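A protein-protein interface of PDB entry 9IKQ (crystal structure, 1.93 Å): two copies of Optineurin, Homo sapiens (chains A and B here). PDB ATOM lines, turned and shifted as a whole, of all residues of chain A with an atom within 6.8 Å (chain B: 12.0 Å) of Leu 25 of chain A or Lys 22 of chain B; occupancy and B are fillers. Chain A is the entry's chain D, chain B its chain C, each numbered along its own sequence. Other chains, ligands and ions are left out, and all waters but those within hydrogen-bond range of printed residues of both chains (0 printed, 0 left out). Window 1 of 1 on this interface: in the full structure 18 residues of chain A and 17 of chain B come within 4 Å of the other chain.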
ATOM      1  N   ARG A  17      11.298 -22.989   9.684  1.00  0.00           N
ATOM      2  CA  ARG A  17      12.330 -22.065  10.152  1.00  0.00           C
ATOM      3  C   ARG A  17      11.797 -20.633  10.263  1.00  0.00           C
ATOM      4  O   ARG A  17      12.027 -19.944  11.262  1.00  0.00           O
ATOM      5  CB  ARG A  17      13.535 -22.135   9.204  1.00  0.00           C
ATOM      6  CG  ARG A  17      14.759 -21.300   9.598  1.00  0.00           C
ATOM      7  CD  ARG A  17      15.564 -20.826   8.360  1.00  0.00           C
ATOM      8  NE  ARG A  17      15.479 -19.375   8.147  1.00  0.00           N
ATOM      9  CZ  ARG A  17      14.987 -18.787   7.056  1.00  0.00           C
ATOM     10  NH1 ARG A  17      14.960 -17.462   6.977  1.00  0.00           N
ATOM     11  NH2 ARG A  17      14.522 -19.513   6.043  1.00  0.00           N
ATOM     12  N   LEU A  18      11.094 -20.164   9.234  1.00  0.00           N
ATOM     13  CA  LEU A  18      10.565 -18.802   9.302  1.00  0.00           C
ATOM     14  C   LEU A  18       9.523 -18.671  10.403  1.00  0.00           C
ATOM     15  O   LEU A  18       9.415 -17.619  11.042  1.00  0.00           O
ATOM     16  CB  LEU A  18       9.965 -18.402   7.955  1.00  0.00           C
ATOM     17  CG  LEU A  18      11.017 -18.124   6.880  1.00  0.00           C
ATOM     18  CD1 LEU A  18      10.398 -18.280   5.504  1.00  0.00           C
ATOM     19  CD2 LEU A  18      11.630 -16.738   7.049  1.00  0.00           C
ATOM     20  N   ALA A  20       9.539 -20.173  13.245  1.00  0.00           N
ATOM     21  CA  ALA A  20      10.221 -20.040  14.524  1.00  0.00           C
ATOM     22  C   ALA A  20      10.833 -18.658  14.666  1.00  0.00           C
ATOM     23  O   ALA A  20      10.791 -18.066  15.751  1.00  0.00           O
ATOM     24  CB  ALA A  20      11.302 -21.114  14.670  1.00  0.00           C
ATOM     25  N   GLU A  21      11.454 -18.152  13.596  1.00  0.00           N
ATOM     26  CA  GLU A  21      11.957 -16.780  13.619  1.00  0.00           C
ATOM     27  C   GLU A  21      10.837 -15.809  13.970  1.00  0.00           C
ATOM     28  O   GLU A  21      10.996 -14.949  14.850  1.00  0.00           O
ATOM     29  CB  GLU A  21      12.589 -16.421  12.269  1.00  0.00           C
ATOM     30  CG  GLU A  21      13.808 -17.273  11.909  1.00  0.00           C
ATOM     31  CD  GLU A  21      14.248 -17.098  10.459  1.00  0.00           C
ATOM     32  OE1 GLU A  21      13.580 -16.363   9.702  1.00  0.00           O
ATOM     33  OE2 GLU A  21      15.279 -17.671  10.093  1.00  0.00           O
ATOM     34  N   LYS A  22       9.669 -15.982  13.351  1.00  0.00           N
ATOM     35  CA  LYS A  22       8.544 -15.099  13.639  1.00  0.00           C
ATOM     36  C   LYS A  22       8.157 -15.160  15.116  1.00  0.00           C
ATOM     37  O   LYS A  22       7.938 -14.126  15.758  1.00  0.00           O
ATOM     38  CB  LYS A  22       7.348 -15.460  12.753  1.00  0.00           C
ATOM     39  CG  LYS A  22       6.082 -14.635  13.082  1.00  0.00           C
ATOM     40  CD  LYS A  22       4.937 -14.987  12.136  1.00  0.00           C
ATOM     41  CE  LYS A  22       3.725 -14.091  12.371  1.00  0.00           C
ATOM     42  NZ  LYS A  22       2.660 -14.553  11.503  1.00  0.00           N
ATOM     43  N   ALA A  23       8.072 -16.370  15.672  1.00  0.00           N
ATOM     44  CA  ALA A  23       7.685 -16.516  17.072  1.00  0.00           C
ATOM     45  C   ALA A  23       8.629 -15.751  17.984  1.00  0.00           C
ATOM     46  O   ALA A  23       8.191 -15.023  18.883  1.00  0.00           O
ATOM     47  CB  ALA A  23       7.650 -17.995  17.463  1.00  0.00           C
ATOM     48  N   ASP A  24       9.936 -15.923  17.785  1.00  0.00           N
ATOM     49  CA  ASP A  24      10.900 -15.185  18.591  1.00  0.00           C
ATOM     50  C   ASP A  24      10.736 -13.682  18.406  1.00  0.00           C
ATOM     51  O   ASP A  24      10.720 -12.921  19.382  1.00  0.00           O
ATOM     52  CB  ASP A  24      12.325 -15.608  18.221  1.00  0.00           C
ATOM     53  CG  ASP A  24      12.706 -16.938  18.841  1.00  0.00           C
ATOM     54  OD1 ASP A  24      11.780 -17.662  19.271  1.00  0.00           O
ATOM     55  OD2 ASP A  24      13.922 -17.249  18.910  1.00  0.00           O
ATOM     56  N   LEU A  25      10.644 -13.238  17.150  1.00  0.00           N
ATOM     57  CA  LEU A  25      10.533 -11.812  16.880  1.00  0.00           C
ATOM     58  C   LEU A  25       9.306 -11.215  17.563  1.00  0.00           C
ATOM     59  O   LEU A  25       9.375 -10.111  18.104  1.00  0.00           O
ATOM     60  CB  LEU A  25      10.494 -11.565  15.375  1.00  0.00           C
ATOM     61  CG  LEU A  25      11.805 -11.838  14.649  1.00  0.00           C
ATOM     62  CD1 LEU A  25      11.623 -11.731  13.129  1.00  0.00           C
ATOM     63  CD2 LEU A  25      12.846 -10.853  15.127  1.00  0.00           C
ATOM     64  N   LEU A  26       8.180 -11.930  17.560  1.00  0.00           N
ATOM     65  CA  LEU A  26       6.982 -11.412  18.220  1.00  0.00           C
ATOM     66  C   LEU A  26       7.185 -11.310  19.724  1.00  0.00           C
ATOM     67  O   LEU A  26       6.743 -10.345  20.358  1.00  0.00           O
ATOM     68  CB  LEU A  26       5.782 -12.301  17.911  1.00  0.00           C
ATOM     69  CG  LEU A  26       5.184 -12.206  16.506  1.00  0.00           C
ATOM     70  CD1 LEU A  26       4.182 -13.343  16.317  1.00  0.00           C
ATOM     71  CD2 LEU A  26       4.513 -10.857  16.289  1.00  0.00           C
ATOM     72  N   GLY A  27       7.853 -12.304  20.313  1.00  0.00           N
ATOM     73  CA  GLY A  27       8.221 -12.196  21.709  1.00  0.00           C
ATOM     74  C   GLY A  27       9.072 -10.976  21.983  1.00  0.00           C
ATOM     75  O   GLY A  27       8.881 -10.288  22.994  1.00  0.00           O
ATOM     76  N   ILE A  28      10.032 -10.694  21.092  1.00  0.00           N
ATOM     77  CA  ILE A  28      10.945  -9.573  21.296  1.00  0.00           C
ATOM     78  C   ILE A  28      10.200  -8.242  21.180  1.00  0.00           C
ATOM     79  O   ILE A  28      10.421  -7.323  21.977  1.00  0.00           O
ATOM     80  CB  ILE A  28      12.130  -9.671  20.310  1.00  0.00           C
ATOM     81  CG1 ILE A  28      13.066 -10.842  20.704  1.00  0.00           C
ATOM     82  CG2 ILE A  28      12.913  -8.369  20.290  1.00  0.00           C
ATOM     83  CD1 ILE A  28      14.054 -11.251  19.602  1.00  0.00           C
ATOM     84  N   VAL A  29       9.292  -8.116  20.200  1.00  0.00           N
ATOM     85  CA  VAL A  29       8.491  -6.888  20.092  1.00  0.00           C
ATOM     86  C   VAL A  29       7.674  -6.677  21.362  1.00  0.00           C
ATOM     87  O   VAL A  29       7.605  -5.561  21.898  1.00  0.00           O
ATOM     88  CB  VAL A  29       7.587  -6.913  18.838  1.00  0.00           C
ATOM     89  CG1 VAL A  29       6.596  -5.746  18.845  1.00  0.00           C
ATOM     90  CG2 VAL A  29       8.425  -6.847  17.579  1.00  0.00           C
ATOM     91  N   SER A  30       7.055  -7.748  21.873  1.00  0.00           N
ATOM     92  CA  SER A  30       6.213  -7.615  23.058  1.00  0.00           C
ATOM     93  C   SER A  30       7.013  -7.139  24.259  1.00  0.00           C
ATOM     94  O   SER A  30       6.577  -6.262  25.009  1.00  0.00           O
ATOM     95  CB  SER A  30       5.535  -8.946  23.382  1.00  0.00           C
ATOM     96  OG  SER A  30       4.468  -9.225  22.485  1.00  0.00           O
ATOM     97  N   THR B  13       3.844 -19.939  -1.495  1.00  0.00           N
ATOM     98  CA  THR B  13       3.149 -18.727  -1.048  1.00  0.00           C
ATOM     99  C   THR B  13       3.383 -18.488   0.435  1.00  0.00           C
ATOM    100  O   THR B  13       3.596 -17.343   0.855  1.00  0.00           O
ATOM    101  CB  THR B  13       1.644 -18.817  -1.338  1.00  0.00           C
ATOM    102  OG1 THR B  13       1.153 -20.113  -0.977  1.00  0.00           O
ATOM    103  CG2 THR B  13       1.396 -18.613  -2.813  1.00  0.00           C
ATOM    104  N   GLN B  14       3.338 -19.550   1.239  1.00  0.00           N
ATOM    105  CA  GLN B  14       3.584 -19.431   2.674  1.00  0.00           C
ATOM    106  C   GLN B  14       4.951 -18.794   2.956  1.00  0.00           C
ATOM    107  O   GLN B  14       5.072 -17.904   3.809  1.00  0.00           O
ATOM    108  CB  GLN B  14       3.465 -20.826   3.286  1.00  0.00           C
ATOM    109  CG  GLN B  14       3.362 -20.934   4.796  1.00  0.00           C
ATOM    110  CD  GLN B  14       2.907 -22.334   5.234  1.00  0.00           C
ATOM    111  OE1 GLN B  14       3.139 -23.325   4.535  1.00  0.00           O
ATOM    112  NE2 GLN B  14       2.303 -22.417   6.414  1.00  0.00           N
ATOM    113  N   VAL B  15       5.989 -19.208   2.230  1.00  0.00           N
ATOM    114  CA  VAL B  15       7.315 -18.643   2.446  1.00  0.00           C
ATOM    115  C   VAL B  15       7.317 -17.153   2.138  1.00  0.00           C
ATOM    116  O   VAL B  15       7.807 -16.337   2.928  1.00  0.00           O
ATOM    117  CB  VAL B  15       8.370 -19.396   1.620  1.00  0.00           C
ATOM    118  CG1 VAL B  15       9.707 -18.676   1.685  1.00  0.00           C
ATOM    119  CG2 VAL B  15       8.508 -20.803   2.152  1.00  0.00           C
ATOM    120  N   VAL B  16       6.737 -16.771   0.994  1.00  0.00           N
ATOM    121  CA  VAL B  16       6.681 -15.353   0.642  1.00  0.00           C
ATOM    122  C   VAL B  16       5.981 -14.558   1.729  1.00  0.00           C
ATOM    123  O   VAL B  16       6.486 -13.520   2.187  1.00  0.00           O
ATOM    124  CB  VAL B  16       6.009 -15.157  -0.725  1.00  0.00           C
ATOM    125  CG1 VAL B  16       5.963 -13.674  -1.061  1.00  0.00           C
ATOM    126  CG2 VAL B  16       6.787 -15.907  -1.803  1.00  0.00           C
ATOM    127  N   ARG B  17       4.815 -15.034   2.188  1.00  0.00           N
ATOM    128  CA  ARG B  17       4.060 -14.318   3.208  1.00  0.00           C
ATOM    129  C   ARG B  17       4.865 -14.177   4.494  1.00  0.00           C
ATOM    130  O   ARG B  17       4.873 -13.116   5.125  1.00  0.00           O
ATOM    131  CB  ARG B  17       2.744 -15.041   3.486  1.00  0.00           C
ATOM    132  CG  ARG B  17       1.924 -14.456   4.616  1.00  0.00           C
ATOM    133  CD  ARG B  17       0.781 -15.397   5.008  1.00  0.00           C
ATOM    134  NE  ARG B  17      -0.176 -15.599   3.925  1.00  0.00           N
ATOM    135  CZ  ARG B  17      -0.382 -16.761   3.308  1.00  0.00           C
ATOM    136  NH1 ARG B  17      -1.288 -16.843   2.340  1.00  0.00           N
ATOM    137  NH2 ARG B  17       0.310 -17.844   3.658  1.00  0.00           N
ATOM    138  N   LEU B  18       5.545 -15.266   4.895  1.00  0.00           N
ATOM    139  CA  LEU B  18       6.332 -15.240   6.127  1.00  0.00           C
ATOM    140  C   LEU B  18       7.547 -14.341   5.994  1.00  0.00           C
ATOM    141  O   LEU B  18       7.941 -13.691   6.965  1.00  0.00           O
ATOM    142  CB  LEU B  18       6.789 -16.652   6.510  1.00  0.00           C
ATOM    143  CG  LEU B  18       5.724 -17.553   7.135  1.00  0.00           C
ATOM    144  CD1 LEU B  18       6.169 -18.989   7.063  1.00  0.00           C
ATOM    145  CD2 LEU B  18       5.407 -17.146   8.577  1.00  0.00           C
ATOM    146  N   GLN B  19       8.162 -14.290   4.813  1.00  0.00           N
ATOM    147  CA  GLN B  19       9.321 -13.414   4.656  1.00  0.00           C
ATOM    148  C   GLN B  19       8.905 -11.954   4.764  1.00  0.00           C
ATOM    149  O   GLN B  19       9.619 -11.148   5.375  1.00  0.00           O
ATOM    150  CB  GLN B  19      10.024 -13.679   3.323  1.00  0.00           C
ATOM    151  CG  GLN B  19      10.753 -15.003   3.298  1.00  0.00           C
ATOM    152  CD  GLN B  19      11.332 -15.354   1.934  1.00  0.00           C
ATOM    153  OE1 GLN B  19      10.708 -15.119   0.890  1.00  0.00           O
ATOM    154  NE2 GLN B  19      12.537 -15.918   1.941  1.00  0.00           N
ATOM    155  N   ALA B  20       7.742 -11.598   4.192  1.00  0.00           N
ATOM    156  CA  ALA B  20       7.288 -10.210   4.283  1.00  0.00           C
ATOM    157  C   ALA B  20       6.967  -9.844   5.728  1.00  0.00           C
ATOM    158  O   ALA B  20       7.308  -8.749   6.192  1.00  0.00           O
ATOM    159  CB  ALA B  20       6.068  -9.986   3.378  1.00  0.00           C
ATOM    160  N   GLU B  21       6.351 -10.772   6.464  1.00  0.00           N
ATOM    161  CA  GLU B  21       6.105 -10.558   7.889  1.00  0.00           C
ATOM    162  C   GLU B  21       7.406 -10.354   8.647  1.00  0.00           C
ATOM    163  O   GLU B  21       7.514  -9.455   9.496  1.00  0.00           O
ATOM    164  CB  GLU B  21       5.338 -11.746   8.473  1.00  0.00           C
ATOM    165  CG  GLU B  21       3.896 -11.885   7.950  1.00  0.00           C
ATOM    166  CD  GLU B  21       3.274 -13.199   8.367  1.00  0.00           C
ATOM    167  OE1 GLU B  21       3.953 -13.960   9.098  1.00  0.00           O
ATOM    168  OE2 GLU B  21       2.115 -13.476   7.974  1.00  0.00           O
ATOM    169  N   LYS B  22       8.400 -11.191   8.359  1.00  0.00           N
ATOM    170  CA  LYS B  22       9.692 -11.086   9.023  1.00  0.00           C
ATOM    171  C   LYS B  22      10.352  -9.742   8.747  1.00  0.00           C
ATOM    172  O   LYS B  22      10.906  -9.120   9.660  1.00  0.00           O
ATOM    173  CB  LYS B  22      10.603 -12.217   8.565  1.00  0.00           C
ATOM    174  CG  LYS B  22      12.019 -12.149   9.177  1.00  0.00           C
ATOM    175  CD  LYS B  22      12.873 -13.329   8.695  1.00  0.00           C
ATOM    176  CE  LYS B  22      14.305 -13.208   9.155  1.00  0.00           C
ATOM    177  NZ  LYS B  22      15.083 -14.435   8.812  1.00  0.00           N
ATOM    178  N   ALA B  23      10.309  -9.280   7.496  1.00  0.00           N
ATOM    179  CA  ALA B  23      10.914  -7.990   7.173  1.00  0.00           C
ATOM    180  C   ALA B  23      10.296  -6.865   7.998  1.00  0.00           C
ATOM    181  O   ALA B  23      11.012  -5.999   8.514  1.00  0.00           O
ATOM    182  CB  ALA B  23      10.785  -7.696   5.678  1.00  0.00           C
ATOM    183  N   ASP B  24       8.964  -6.850   8.125  1.00  0.00           N
ATOM    184  CA  ASP B  24       8.321  -5.808   8.918  1.00  0.00           C
ATOM    185  C   ASP B  24       8.704  -5.918  10.382  1.00  0.00           C
ATOM    186  O   ASP B  24       9.011  -4.914  11.029  1.00  0.00           O
ATOM    187  CB  ASP B  24       6.807  -5.873   8.760  1.00  0.00           C
ATOM    188  CG  ASP B  24       6.345  -5.254   7.453  1.00  0.00           C
ATOM    189  OD1 ASP B  24       7.213  -5.029   6.578  1.00  0.00           O
ATOM    190  OD2 ASP B  24       5.129  -4.962   7.308  1.00  0.00           O
ATOM    191  N   LEU B  25       8.679  -7.136  10.931  1.00  0.00           N
ATOM    192  CA  LEU B  25       8.990  -7.285  12.350  1.00  0.00           C
ATOM    193  C   LEU B  25      10.412  -6.819  12.655  1.00  0.00           C
ATOM    194  O   LEU B  25      10.647  -6.165  13.678  1.00  0.00           O
ATOM    195  CB  LEU B  25       8.794  -8.737  12.788  1.00  0.00           C
ATOM    196  CG  LEU B  25       7.340  -9.202  12.757  1.00  0.00           C
ATOM    197  CD1 LEU B  25       7.237 -10.722  12.977  1.00  0.00           C
ATOM    198  CD2 LEU B  25       6.527  -8.424  13.805  1.00  0.00           C
ATOM    199  N   LEU B  26      11.374  -7.159  11.787  1.00  0.00           N
ATOM    200  CA  LEU B  26      12.761  -6.736  12.001  1.00  0.00           C
ATOM    201  C   LEU B  26      12.855  -5.216  12.049  1.00  0.00           C
ATOM    202  O   LEU B  26      13.507  -4.644  12.931  1.00  0.00           O
ATOM    203  CB  LEU B  26      13.669  -7.289  10.898  1.00  0.00           C
ATOM    204  CG  LEU B  26      13.931  -8.793  10.860  1.00  0.00           C
ATOM    205  CD1 LEU B  26      14.700  -9.178   9.603  1.00  0.00           C
ATOM    206  CD2 LEU B  26      14.708  -9.219  12.092  1.00  0.00           C
ATOM    207  N   GLY B  27      12.207  -4.545  11.096  1.00  0.00           N
ATOM    208  CA  GLY B  27      12.147  -3.093  11.144  1.00  0.00           C
ATOM    209  C   GLY B  27      11.549  -2.575  12.437  1.00  0.00           C
ATOM    210  O   GLY B  27      12.012  -1.578  12.983  1.00  0.00           O
ATOM    211  N   ILE B  28      10.529  -3.263  12.952  1.00  0.00           N
ATOM    212  CA  ILE B  28       9.869  -2.820  14.177  1.00  0.00           C
ATOM    213  C   ILE B  28      10.779  -3.011  15.389  1.00  0.00           C
ATOM    214  O   ILE B  28      10.878  -2.138  16.263  1.00  0.00           O
ATOM    215  CB  ILE B  28       8.527  -3.556  14.340  1.00  0.00           C
ATOM    216  CG1 ILE B  28       7.509  -2.993  13.336  1.00  0.00           C
ATOM    217  CG2 ILE B  28       8.030  -3.467  15.788  1.00  0.00           C
ATOM    218  CD1 ILE B  28       6.285  -3.874  13.124  1.00  0.00           C
ATOM    219  N   VAL B  29      11.445  -4.159  15.469  1.00  0.00           N
ATOM    220  CA  VAL B  29      12.427  -4.379  16.529  1.00  0.00           C
ATOM    221  C   VAL B  29      13.496  -3.293  16.496  1.00  0.00           C
ATOM    222  O   VAL B  29      13.816  -2.683  17.526  1.00  0.00           O
ATOM    223  CB  VAL B  29      13.038  -5.788  16.402  1.00  0.00           C
ATOM    224  CG1 VAL B  29      14.281  -5.922  17.297  1.00  0.00           C
ATOM    225  CG2 VAL B  29      11.972  -6.864  16.763  1.00  0.00           C
ATOM    226  N   SER B  30      14.045  -3.010  15.301  1.00  0.00           N
ATOM    227  CA  SER B  30      15.127  -2.026  15.189  1.00  0.00           C
ATOM    228  C   SER B  30      14.701  -0.667  15.682  1.00  0.00           C
ATOM    229  O   SER B  30      15.440   0.042  16.377  1.00  0.00           O
ATOM    230  CB  SER B  30      15.609  -1.917  13.738  1.00  0.00           C
ATOM    231  OG  SER B  30      16.390  -3.026  13.346  1.00  0.00           O
ATOM    232  N   GLU B  31      13.468  -0.232  15.354  1.00  0.00           N
ATOM    233  CA  GLU B  31      13.044   1.098  15.755  1.00  0.00           C
ATOM    234  C   GLU B  31      12.733   1.156  17.251  1.00  0.00           C
ATOM    235  O   GLU B  31      13.065   2.142  17.920  1.00  0.00           O
ATOM    236  CB  GLU B  31      11.846   1.544  14.915  1.00  0.00           C
ATOM    237  CG  GLU B  31      12.216   1.918  13.472  1.00  0.00           C
ATOM    238  CD  GLU B  31      13.395   2.880  13.373  1.00  0.00           C
ATOM    239  OE1 GLU B  31      13.250   4.055  13.769  1.00  0.00           O
ATOM    240  OE2 GLU B  31      14.472   2.471  12.893  1.00  0.00           O
ATOM    241  N   LEU B  32      12.118   0.100  17.799  1.00  0.00           N
ATOM    242  CA  LEU B  32      11.873   0.059  19.237  1.00  0.00           C
ATOM    243  C   LEU B  32      13.174   0.158  20.028  1.00  0.00           C
ATOM    244  O   LEU B  32      13.236   0.882  21.026  1.00  0.00           O
ATOM    245  CB  LEU B  32      11.120  -1.223  19.608  1.00  0.00           C
ATOM    246  CG  LEU B  32       9.671  -1.312  19.109  1.00  0.00           C
ATOM    247  CD1 LEU B  32       9.062  -2.663  19.451  1.00  0.00           C
ATOM    248  CD2 LEU B  32       8.832  -0.184  19.699  1.00  0.00           C
ATOM    249  N   GLN B  33      14.225  -0.559  19.596  1.00  0.00           N
ATOM    250  CA  GLN B  33      15.493  -0.512  20.326  1.00  0.00           C
ATOM    251  C   GLN B  33      16.084   0.889  20.306  1.00  0.00           C
ATOM    252  O   GLN B  33      16.695   1.323  21.289  1.00  0.00           O
ATOM    253  CB  GLN B  33      16.499  -1.521  19.759  1.00  0.00           C
ATOM    254  CG  GLN B  33      16.022  -2.947  19.869  1.00  0.00           C
ATOM    255  CD  GLN B  33      17.127  -3.978  19.675  1.00  0.00           C
ATOM    256  OE1 GLN B  33      17.201  -4.950  20.423  1.00  0.00           O
ATOM    257  NE2 GLN B  33      17.969  -3.786  18.659  1.00  0.00           N
ATOM    258  N   LEU B  36      14.400   2.956  23.018  1.00  0.00           N
ATOM    259  CA  LEU B  36      14.901   2.618  24.345  1.00  0.00           C
ATOM    260  C   LEU B  36      16.308   3.128  24.591  1.00  0.00           C
ATOM    261  O   LEU B  36      16.740   3.172  25.748  1.00  0.00           O
ATOM    262  CB  LEU B  36      14.906   1.103  24.530  1.00  0.00           C
ATOM    263  CG  LEU B  36      13.575   0.376  24.649  1.00  0.00           C
ATOM    264  CD1 LEU B  36      13.811  -1.111  24.540  1.00  0.00           C
ATOM    265  CD2 LEU B  36      12.950   0.703  25.987  1.00  0.00           C
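Of the printed residues of chain B, Leu 18 of chain A touches Val 15 (3.9 Å), Leu 18 (3.9 Å), Gln 19 (3.97 Å) and Lys 22 (3.98 Å). Glu 21 of chain A touches one residue of chain B. No residue of chain B comes within 4 Å of Ala 23 of chain A. No residue of chain B comes within 4 Å of Asp 24 of chain A. Printed residues of chain B within 4 Å of Leu 25 of chain A: Lys 22 and Leu 26. No residue of chain B comes within 4 Å of Gly 27 of chain A. Gln 14 of chain B touches none of the printed residues of chain A. Of the printed residues of chain A, Val 15 of chain B touches Leu 18 (3.9 Å). Arg 17 of chain B touches none of the printed residues of chain A. Printed residues of chain A within 4 Å of Lys 22 of chain B: Arg 17, Leu 18, Glu 21 and Leu 25. The nearest printed residue of chain B that does not touch Val 29 of chain A is Leu 25 of chain B (4.5 Å).
Leu 18 of chain A touches its own counterpart, Leu 18 of chain B. Leu 18 of chain A touches Lys 22 of chain B, but with the chains exchanged Lys 22 of chain A does not touch Leu 18 of chain B (4.2 Å). Leu 25 of chain A touches Lys 22 of chain B, but with the chains exchanged Lys 22 of chain A does not touch Leu 25 of chain B (4.1 Å). Val 29 of chain A touches its own counterpart, Val 29 of chain B. Positions printed for both chains: 17, 18, 20, 21, 22, 23, 24, 25, 26, 27, 28, 29 and 30. Of the 13 pairs that touch across the chains among the printed residues, 6 have their exchanged pair printed and touching as well.
The side-chain amino group of Lys 22 of chain B is in salt-bridge range of the side-chain carboxylate of Glu 21 of chain A (2.6 Å). NZ of Lys 22 of chain A lies within salt-bridge range of OE1 of Glu 21 of chain B (2.8 Å).
Of the 22 printed residues of chain B, 9 touch a printed residue of chain A. Hydrophobic or aromatic side chains of chain B within 4 Å of the printed part of chain A: Val 15, Leu 18, Leu 26, Ile 28, Val 29 and Leu 32.
Lys 22 of chain B touches Arg 17 of chain A (NZ to NH1, 3.5 Å). Leu 18 of chain A touches Val 15 of chain B (CD1 to CG1, 3.9 Å). Leu 18 of chain A touches Gln 19 of chain B (CD1 to CG, 3.97 Å). Leu 18 of chain A touches Lys 22 of chain B. CD1 of Leu 25 of chain A touches CG of Lys 22 of chain B (3.99 Å). Leu 25 of chain A touches Leu 26 of chain B (CD2 to CD2, 3.9 Å). CG2 of Ile 28 of chain A touches CG2 of Val 29 of chain B, 3.9 Å away. Ile 28 of chain B touches Val 29 of chain A. Val 29 of chain B touches Val 29 of chain A (CG2 to CG2, 3.6 Å). Val 29 of chain A touches Leu 32 of chain B.
The side-chain carboxylate of Glu 21 of chain A lies within salt-bridge range of the guanidinium group of Arg 17 of chain A. The backbone carbonyl oxygen of Leu 26 of chain B lies within hydrogen-bond range of the side-chain hydroxyl of Ser 30 of chain B (3.3 Å).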
